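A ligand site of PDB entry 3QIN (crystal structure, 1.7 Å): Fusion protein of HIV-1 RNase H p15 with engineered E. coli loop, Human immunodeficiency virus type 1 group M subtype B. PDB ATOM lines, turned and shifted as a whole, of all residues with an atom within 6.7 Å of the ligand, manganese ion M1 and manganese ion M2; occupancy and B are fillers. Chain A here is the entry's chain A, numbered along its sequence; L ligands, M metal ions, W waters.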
ATOM      1  N   VAL A  17     -20.865  12.945   4.683  1.00  0.00           N
ATOM      2  CA  VAL A  17     -22.242  13.137   5.095  1.00  0.00           C
ATOM      3  C   VAL A  17     -22.760  14.459   4.583  1.00  0.00           C
ATOM      4  O   VAL A  17     -21.988  15.376   4.332  1.00  0.00           O
ATOM      5  CB  VAL A  17     -22.409  13.096   6.646  1.00  0.00           C
ATOM      6  CG1 VAL A  17     -22.184  11.686   7.206  1.00  0.00           C
ATOM      7  CG2 VAL A  17     -21.487  14.100   7.363  1.00  0.00           C
ATOM      8  N   ASP A  18     -24.070  14.550   4.416  1.00  0.00           N
ATOM      9  CA  ASP A  18     -24.686  15.835   4.094  1.00  0.00           C
ATOM     10  C   ASP A  18     -26.177  15.744   4.307  1.00  0.00           C
ATOM     11  O   ASP A  18     -26.727  14.670   4.470  1.00  0.00           O
ATOM     12  CB  ASP A  18     -24.384  16.233   2.647  1.00  0.00           C
ATOM     13  CG  ASP A  18     -24.571  17.712   2.397  1.00  0.00           C
ATOM     14  OD1 ASP A  18     -24.574  18.507   3.374  1.00  0.00           O
ATOM     15  OD2 ASP A  18     -24.725  18.088   1.218  1.00  0.00           O
ATOM     16  N   GLY A  19     -26.832  16.908   4.336  1.00  0.00           N
ATOM     17  CA  GLY A  19     -28.270  16.950   4.435  1.00  0.00           C
ATOM     18  C   GLY A  19     -28.808  18.120   3.643  1.00  0.00           C
ATOM     19  O   GLY A  19     -28.085  19.079   3.335  1.00  0.00           O
ATOM     20  N   ALA A  20     -30.089  18.029   3.296  1.00  0.00           N
ATOM     21  CA  ALA A  20     -30.778  19.120   2.619  1.00  0.00           C
ATOM     22  C   ALA A  20     -32.211  19.109   3.125  1.00  0.00           C
ATOM     23  O   ALA A  20     -32.768  18.051   3.429  1.00  0.00           O
ATOM     24  CB  ALA A  20     -30.740  18.936   1.110  1.00  0.00           C
ATOM     25  N   ASN A  49     -32.326  22.285   7.522  1.00  0.00           N
ATOM     26  CA  ASN A  49     -30.994  22.027   6.994  1.00  0.00           C
ATOM     27  C   ASN A  49     -30.051  21.598   8.121  1.00  0.00           C
ATOM     28  O   ASN A  49     -29.393  20.556   8.016  1.00  0.00           O
ATOM     29  CB  ASN A  49     -30.449  23.236   6.226  1.00  0.00           C
ATOM     30  CG  ASN A  49     -31.057  23.367   4.834  1.00  0.00           C
ATOM     31  OD1 ASN A  49     -30.996  22.443   4.012  1.00  0.00           O
ATOM     32  ND2 ASN A  49     -31.637  24.537   4.557  1.00  0.00           N
ATOM     33  N   GLU A  53     -28.230  17.677   8.827  1.00  0.00           N
ATOM     34  CA  GLU A  53     -26.786  17.480   8.890  1.00  0.00           C
ATOM     35  C   GLU A  53     -26.429  16.627  10.104  1.00  0.00           C
ATOM     36  O   GLU A  53     -25.584  15.739  10.006  1.00  0.00           O
ATOM     37  CB  GLU A  53     -26.071  18.829   8.970  1.00  0.00           C
ATOM     38  CG  GLU A  53     -26.278  19.701   7.734  1.00  0.00           C
ATOM     39  CD  GLU A  53     -25.307  19.403   6.601  1.00  0.00           C
ATOM     40  OE1 GLU A  53     -25.335  20.144   5.604  1.00  0.00           O
ATOM     41  OE2 GLU A  53     -24.481  18.459   6.718  1.00  0.00           O
ATOM     42  N   THR A  72     -17.825  16.211   7.157  1.00  0.00           N
ATOM     43  CA  THR A  72     -19.006  17.041   7.022  1.00  0.00           C
ATOM     44  C   THR A  72     -18.635  18.371   6.392  1.00  0.00           C
ATOM     45  O   THR A  72     -17.496  18.797   6.478  1.00  0.00           O
ATOM     46  CB  THR A  72     -19.645  17.286   8.409  1.00  0.00           C
ATOM     47  OG1 THR A  72     -20.860  18.031   8.242  1.00  0.00           O
ATOM     48  CG2 THR A  72     -18.688  18.101   9.301  1.00  0.00           C
ATOM     49  N   ASP A  73     -19.601  19.021   5.733  1.00  0.00           N
ATOM     50  CA  ASP A  73     -19.385  20.403   5.255  1.00  0.00           C
ATOM     51  C   ASP A  73     -20.183  21.424   6.075  1.00  0.00           C
ATOM     52  O   ASP A  73     -20.181  22.632   5.768  1.00  0.00           O
ATOM     53  CB  ASP A  73     -19.625  20.532   3.746  1.00  0.00           C
ATOM     54  CG  ASP A  73     -21.054  20.258   3.325  1.00  0.00           C
ATOM     55  OD1 ASP A  73     -21.275  19.942   2.146  1.00  0.00           O
ATOM     56  OD2 ASP A  73     -21.946  20.389   4.157  1.00  0.00           O
ATOM     57  N   SER A  74     -20.825  20.943   7.128  1.00  0.00           N
ATOM     58  CA  SER A  74     -21.649  21.785   7.986  1.00  0.00           C
ATOM     59  C   SER A  74     -20.854  22.433   9.126  1.00  0.00           C
ATOM     60  O   SER A  74     -20.396  21.730  10.032  1.00  0.00           O
ATOM     61  CB  SER A  74     -22.802  20.968   8.587  1.00  0.00           C
ATOM     62  OG  SER A  74     -23.577  21.753   9.491  1.00  0.00           O
ATOM     63  N   GLN A  75     -20.714  23.754   9.074  1.00  0.00           N
ATOM     64  CA  GLN A  75     -20.126  24.505  10.183  1.00  0.00           C
ATOM     65  C   GLN A  75     -20.906  24.236  11.471  1.00  0.00           C
ATOM     66  O   GLN A  75     -20.325  24.054  12.541  1.00  0.00           O
ATOM     67  CB  GLN A  75     -20.142  26.014   9.894  1.00  0.00           C
ATOM     68  CG  GLN A  75     -19.324  26.457   8.685  1.00  0.00           C
ATOM     69  CD  GLN A  75     -19.145  27.971   8.665  1.00  0.00           C
ATOM     70  OE1 GLN A  75     -18.321  28.510   9.422  1.00  0.00           O
ATOM     71  NE2 GLN A  75     -19.922  28.665   7.833  1.00  0.00           N
ATOM     72  N   TYR A  76     -22.228  24.253  11.362  1.00  0.00           N
ATOM     73  CA  TYR A  76     -23.067  24.071  12.539  1.00  0.00           C
ATOM     74  C   TYR A  76     -22.890  22.697  13.158  1.00  0.00           C
ATOM     75  O   TYR A  76     -22.675  22.572  14.370  1.00  0.00           O
ATOM     76  CB  TYR A  76     -24.537  24.262  12.160  1.00  0.00           C
ATOM     77  CG  TYR A  76     -25.471  23.733  13.217  1.00  0.00           C
ATOM     78  CD1 TYR A  76     -25.705  24.433  14.392  1.00  0.00           C
ATOM     79  CD2 TYR A  76     -26.142  22.520  13.035  1.00  0.00           C
ATOM     80  CE1 TYR A  76     -26.558  23.961  15.355  1.00  0.00           C
ATOM     81  CE2 TYR A  76     -26.996  22.035  14.001  1.00  0.00           C
ATOM     82  CZ  TYR A  76     -27.209  22.758  15.157  1.00  0.00           C
ATOM     83  OH  TYR A  76     -28.063  22.279  16.114  1.00  0.00           O
ATOM     84  N   TRP A 124     -14.162  18.869   8.831  1.00  0.00           N
ATOM     85  CA  TRP A 124     -14.961  19.758   7.995  1.00  0.00           C
ATOM     86  C   TRP A 124     -14.261  20.050   6.698  1.00  0.00           C
ATOM     87  O   TRP A 124     -13.042  20.246   6.671  1.00  0.00           O
ATOM     88  CB  TRP A 124     -15.198  21.093   8.715  1.00  0.00           C
ATOM     89  CG  TRP A 124     -15.952  22.105   7.926  1.00  0.00           C
ATOM     90  CD1 TRP A 124     -17.298  22.251   7.878  1.00  0.00           C
ATOM     91  CD2 TRP A 124     -15.395  23.144   7.106  1.00  0.00           C
ATOM     92  NE1 TRP A 124     -17.621  23.308   7.061  1.00  0.00           N
ATOM     93  CE2 TRP A 124     -16.476  23.876   6.584  1.00  0.00           C
ATOM     94  CE3 TRP A 124     -14.084  23.527   6.771  1.00  0.00           C
ATOM     95  CZ2 TRP A 124     -16.296  24.982   5.745  1.00  0.00           C
ATOM     96  CZ3 TRP A 124     -13.905  24.619   5.935  1.00  0.00           C
ATOM     97  CH2 TRP A 124     -15.007  25.333   5.425  1.00  0.00           C
ATOM     98  N   PRO A 126     -15.130  22.434   2.920  1.00  0.00           N
ATOM     99  CA  PRO A 126     -16.052  23.427   2.355  1.00  0.00           C
ATOM    100  C   PRO A 126     -17.023  22.789   1.376  1.00  0.00           C
ATOM    101  O   PRO A 126     -16.639  21.939   0.582  1.00  0.00           O
ATOM    102  CB  PRO A 126     -15.124  24.416   1.638  1.00  0.00           C
ATOM    103  CG  PRO A 126     -13.855  23.691   1.424  1.00  0.00           C
ATOM    104  CD  PRO A 126     -13.733  22.733   2.579  1.00  0.00           C
ATOM    105  N   ALA A 127     -18.277  23.210   1.450  1.00  0.00           N
ATOM    106  CA  ALA A 127     -19.291  22.746   0.501  1.00  0.00           C
ATOM    107  C   ALA A 127     -19.034  23.260  -0.918  1.00  0.00           C
ATOM    108  O   ALA A 127     -18.504  24.357  -1.113  1.00  0.00           O
ATOM    109  CB  ALA A 127     -20.678  23.184   0.979  1.00  0.00           C
ATOM    110  N   HIS A 128     -19.403  22.435  -1.894  1.00  0.00           N
ATOM    111  CA  HIS A 128     -19.429  22.863  -3.289  1.00  0.00           C
ATOM    112  C   HIS A 128     -18.077  23.346  -3.797  1.00  0.00           C
ATOM    113  O   HIS A 128     -17.993  24.300  -4.581  1.00  0.00           O
ATOM    114  CB  HIS A 128     -20.543  23.893  -3.496  1.00  0.00           C
ATOM    115  CG  HIS A 128     -21.901  23.339  -3.226  1.00  0.00           C
ATOM    116  ND1 HIS A 128     -22.501  22.433  -4.079  1.00  0.00           N
ATOM    117  CD2 HIS A 128     -22.730  23.459  -2.162  1.00  0.00           C
ATOM    118  CE1 HIS A 128     -23.668  22.070  -3.586  1.00  0.00           C
ATOM    119  NE2 HIS A 128     -23.826  22.664  -2.419  1.00  0.00           N
ATOM    120  N   LYS A 129     -17.026  22.650  -3.383  1.00  0.00           N
ATOM    121  CA  LYS A 129     -15.673  22.908  -3.859  1.00  0.00           C
ATOM    122  C   LYS A 129     -15.031  21.671  -4.486  1.00  0.00           C
ATOM    123  O   LYS A 129     -13.815  21.538  -4.503  1.00  0.00           O
ATOM    124  CB  LYS A 129     -14.774  23.419  -2.737  1.00  0.00           C
ATOM    125  CG  LYS A 129     -15.214  24.747  -2.191  1.00  0.00           C
ATOM    126  CD  LYS A 129     -14.052  25.560  -1.621  1.00  0.00           C
ATOM    127  CE  LYS A 129     -14.404  27.048  -1.616  1.00  0.00           C
ATOM    128  NZ  LYS A 129     -13.399  27.888  -0.911  1.00  0.00           N
ATOM    129  N   ASN A 134     -17.926  14.468  -1.003  1.00  0.00           N
ATOM    130  CA  ASN A 134     -18.849  15.519  -0.584  1.00  0.00           C
ATOM    131  C   ASN A 134     -19.843  15.911  -1.688  1.00  0.00           C
ATOM    132  O   ASN A 134     -21.044  16.051  -1.427  1.00  0.00           O
ATOM    133  CB  ASN A 134     -18.083  16.745  -0.082  1.00  0.00           C
ATOM    134  CG  ASN A 134     -18.983  17.931   0.186  1.00  0.00           C
ATOM    135  OD1 ASN A 134     -19.102  18.832  -0.646  1.00  0.00           O
ATOM    136  ND2 ASN A 134     -19.635  17.930   1.329  1.00  0.00           N
ATOM    137  N   VAL A 137     -22.537  12.966  -2.105  1.00  0.00           N
ATOM    138  CA  VAL A 137     -23.593  12.935  -1.106  1.00  0.00           C
ATOM    139  C   VAL A 137     -24.488  14.168  -1.237  1.00  0.00           C
ATOM    140  O   VAL A 137     -25.700  14.066  -1.064  1.00  0.00           O
ATOM    141  CB  VAL A 137     -23.056  12.738   0.337  1.00  0.00           C
ATOM    142  CG1 VAL A 137     -22.259  13.987   0.819  1.00  0.00           C
ATOM    143  CG2 VAL A 137     -24.222  12.479   1.293  1.00  0.00           C
ATOM    144  N   ASP A 138     -23.907  15.323  -1.561  1.00  0.00           N
ATOM    145  CA  ASP A 138     -24.745  16.506  -1.749  1.00  0.00           C
ATOM    146  C   ASP A 138     -25.794  16.262  -2.864  1.00  0.00           C
ATOM    147  O   ASP A 138     -26.969  16.608  -2.719  1.00  0.00           O
ATOM    148  CB  ASP A 138     -23.921  17.760  -2.078  1.00  0.00           C
ATOM    149  CG  ASP A 138     -24.794  18.924  -2.505  1.00  0.00           C
ATOM    150  OD1 ASP A 138     -25.017  19.091  -3.726  1.00  0.00           O
ATOM    151  OD2 ASP A 138     -25.303  19.618  -1.611  1.00  0.00           O
ATOM    152  N   LYS A 139     -25.365  15.658  -3.963  1.00  0.00           N
ATOM    153  CA  LYS A 139     -26.265  15.356  -5.056  1.00  0.00           C
ATOM    154  C   LYS A 139     -27.424  14.457  -4.605  1.00  0.00           C
ATOM    155  O   LYS A 139     -28.573  14.674  -4.975  1.00  0.00           O
ATOM    156  CB  LYS A 139     -25.509  14.694  -6.202  1.00  0.00           C
ATOM    157  CG  LYS A 139     -26.318  14.495  -7.478  1.00  0.00           C
ATOM    158  CD  LYS A 139     -25.423  14.073  -8.633  1.00  0.00           C
ATOM    159  CE  LYS A 139     -26.187  14.021  -9.954  1.00  0.00           C
ATOM    160  NZ  LYS A 139     -27.210  12.948  -9.975  1.00  0.00           N
ATOM    161  N   VAL A 141     -28.682  13.977  -1.413  1.00  0.00           N
ATOM    162  CA  VAL A 141     -29.636  14.501  -0.443  1.00  0.00           C
ATOM    163  C   VAL A 141     -30.440  15.689  -0.986  1.00  0.00           C
ATOM    164  O   VAL A 141     -31.520  15.997  -0.482  1.00  0.00           O
ATOM    165  CB  VAL A 141     -29.000  14.846   0.914  1.00  0.00           C
ATOM    166  CG1 VAL A 141     -28.258  13.627   1.472  1.00  0.00           C
ATOM    167  CG2 VAL A 141     -28.093  16.092   0.809  1.00  0.00           C
ATOM    168  N   SER A 142     -29.919  16.378  -2.001  1.00  0.00           N
ATOM    169  CA  SER A 142     -30.600  17.575  -2.440  1.00  0.00           C
ATOM    170  C   SER A 142     -31.621  17.264  -3.528  1.00  0.00           C
ATOM    171  O   SER A 142     -32.475  18.080  -3.849  1.00  0.00           O
ATOM    172  CB  SER A 142     -29.597  18.624  -2.926  1.00  0.00           C
ATOM    173  OG  SER A 142     -28.933  18.166  -4.083  1.00  0.00           O
ATOM    174  N   ARG A 146     -33.824  20.309  -2.875  1.00  0.00           N
ATOM    175  CA  ARG A 146     -33.288  21.619  -3.230  1.00  0.00           C
ATOM    176  C   ARG A 146     -33.629  21.953  -4.677  1.00  0.00           C
ATOM    177  O   ARG A 146     -33.273  21.217  -5.588  1.00  0.00           O
ATOM    178  CB  ARG A 146     -31.782  21.667  -3.016  1.00  0.00           C
ATOM    179  CG  ARG A 146     -31.161  23.043  -3.243  1.00  0.00           C
ATOM    180  CD  ARG A 146     -29.657  23.028  -2.987  1.00  0.00           C
ATOM    181  NE  ARG A 146     -28.945  22.165  -3.932  1.00  0.00           N
ATOM    182  CZ  ARG A 146     -27.814  21.517  -3.653  1.00  0.00           C
ATOM    183  NH1 ARG A 146     -27.251  21.614  -2.459  1.00  0.00           N
ATOM    184  NH2 ARG A 146     -27.239  20.762  -4.587  1.00  0.00           N
HETATM  185  C1  LIG L   1     -23.662  27.318  -1.620  1.00  0.00           C
HETATM  186  C2  LIG L   1     -22.627  27.539  -2.506  1.00  0.00           C
HETATM  187  C3  LIG L   1     -21.288  27.345  -2.167  1.00  0.00           C
HETATM  188  C4  LIG L   1     -20.964  26.905  -0.885  1.00  0.00           C
HETATM  189  C5  LIG L   1     -21.987  26.706   0.040  1.00  0.00           C
HETATM  190  C6  LIG L   1     -23.327  26.903  -0.322  1.00  0.00           C
HETATM  191  C7  LIG L   1     -24.421  26.671   0.677  1.00  0.00           C
HETATM  192  C8  LIG L   1     -24.498  25.248   1.153  1.00  0.00           C
HETATM  193  N1  LIG L   1     -24.215  25.035   2.439  1.00  0.00           N
HETATM  194  C9  LIG L   1     -24.289  23.741   2.845  1.00  0.00           C
HETATM  195  C10 LIG L   1     -24.643  22.700   2.013  1.00  0.00           C
HETATM  196  C11 LIG L   1     -24.900  23.071   0.723  1.00  0.00           C
HETATM  197  N2  LIG L   1     -24.839  24.334   0.237  1.00  0.00           N
HETATM  198  O1  LIG L   1     -24.697  21.403   2.405  1.00  0.00           O
HETATM  199  O2  LIG L   1     -25.251  22.143  -0.190  1.00  0.00           O
HETATM  200  C12 LIG L   1     -23.984  23.522   4.283  1.00  0.00           C
HETATM  201  O3  LIG L   1     -23.639  24.684   4.859  1.00  0.00           O
HETATM  202  O4  LIG L   1     -24.065  22.472   4.884  1.00  0.00           O
HETATM  203 BR1  LIG L   1     -23.023  28.142  -4.268  1.00  0.00          BR
HETATM  204  O5  LIG L   1     -20.365  27.563  -3.151  1.00  0.00           O
HETATM  205  C13 LIG L   1     -18.982  27.448  -2.808  1.00  0.00           C
HETATM  206 MN    MN M   1     -24.069  20.407   4.017  1.00  0.00          MN
HETATM  207 MN    MN M   2     -25.021  20.070   0.449  1.00  0.00          MN
HETATM  208  O   HOH W   1     -17.785  26.521   0.424  1.00  0.00           O
HETATM  209  O   HOH W   2     -22.843  20.334   0.211  1.00  0.00           O
HETATM  210  O   HOH W   3     -27.208  20.017   0.896  1.00  0.00           O
HETATM  211  O   HOH W   4     -23.538  27.773   3.707  1.00  0.00           O
HETATM  212  O   HOH W   5     -24.925  23.172   7.527  1.00  0.00           O
HETATM  213  O   HOH W   6     -27.187  24.837  -1.297  1.00  0.00           O
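The guanidinium group of Arg 146 lies within hydrogen-bond range of the side-chain hydroxyl of Ser 142 (3.1 Å). The indole nitrogen of Trp 124 sits at hydrogen-bond distance from the backbone carbonyl oxygen of Asp 73, 2.9 Å away. The backbone NH of Ser 74 is in hydrogen-bond range of the side-chain hydroxyl of Thr 72, at 3.1 Å. The side-chain carboxylate of Asp 138 lies close to a ring nitrogen (NE2) of His 128, 3.5 Å away. The backbone carbonyl oxygen (O) of Asp 138 sits at hydrogen-bond distance from the side-chain hydroxyl (OG) of Ser 142, 2.9 Å away. The backbone NH (N) of Tyr 76 sits close to the side-chain hydroxyl (OG) of Ser 74 (3.4 Å). OD1 of Asp 73 is in hydrogen-bond range of ND2 of Asn 134, 2.7 Å away. OD1 of Asp 138 lies within salt-bridge range of NH2 of Arg 146.
Merely in contact with manganese ion M2: Arg 146 (3.98 Å). The nearest printed residue that does not touch manganese ion M2 is His 128 (4.05 Å).
Water W6 bridges a nitrogen (N2) of the ligand (2.8 Å) and the guanidinium group (NH1) of Arg 146 (3.4 Å). Water W5 lies within hydrogen-bond range of the side-chain hydroxyl of Ser 74 (2.8 Å) and an oxygen (O3) of the ligand (3.3 Å).
Manganese ion M2 is bound by OD2 of Asp 138 (2.1 Å), OD2 of Asp 18 (2.1 Å), O2 of the ligand (2.2 Å), water W2 (2.2 Å), water W3 (2.2 Å) and O1 of the ligand (2.4 Å). Manganese ion M2 has six donor atoms within binding distance.
Manganese ion M1 is bound by O1 of the ligand (2.0 Å). Manganese ion M1 is bound by OE1 of Glu 53 (2.0 Å). OD1 of Asp 18 binds manganese ion M1, 2.1 Å away. Manganese ion M1 is bound by OD2 of Asp 73. Manganese ion M1 is bound by O4 of the ligand (2.2 Å).
An oxygen (O2) of the ligand lies close to the guanidinium group (NH1) of Arg 146, 3.1 Å away. N2 of the ligand sits at hydrogen-bond distance from NE2 of His 128, at 3.3 Å.
Residues that only touch the ligand: Ser 74 (3.99 Å) and Ala 127 (3.5 Å). Within 4 Å of the ligand: Asp 18, Glu 53, Asp 73, Ser 74, Ala 127, His 128, Asp 138 and Arg 146. The nearest printed residue that does not touch the ligand is Gly 19 (4.2 Å).
Of the 23 residues printed, 3 come within 4 Å of manganese ion M1.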
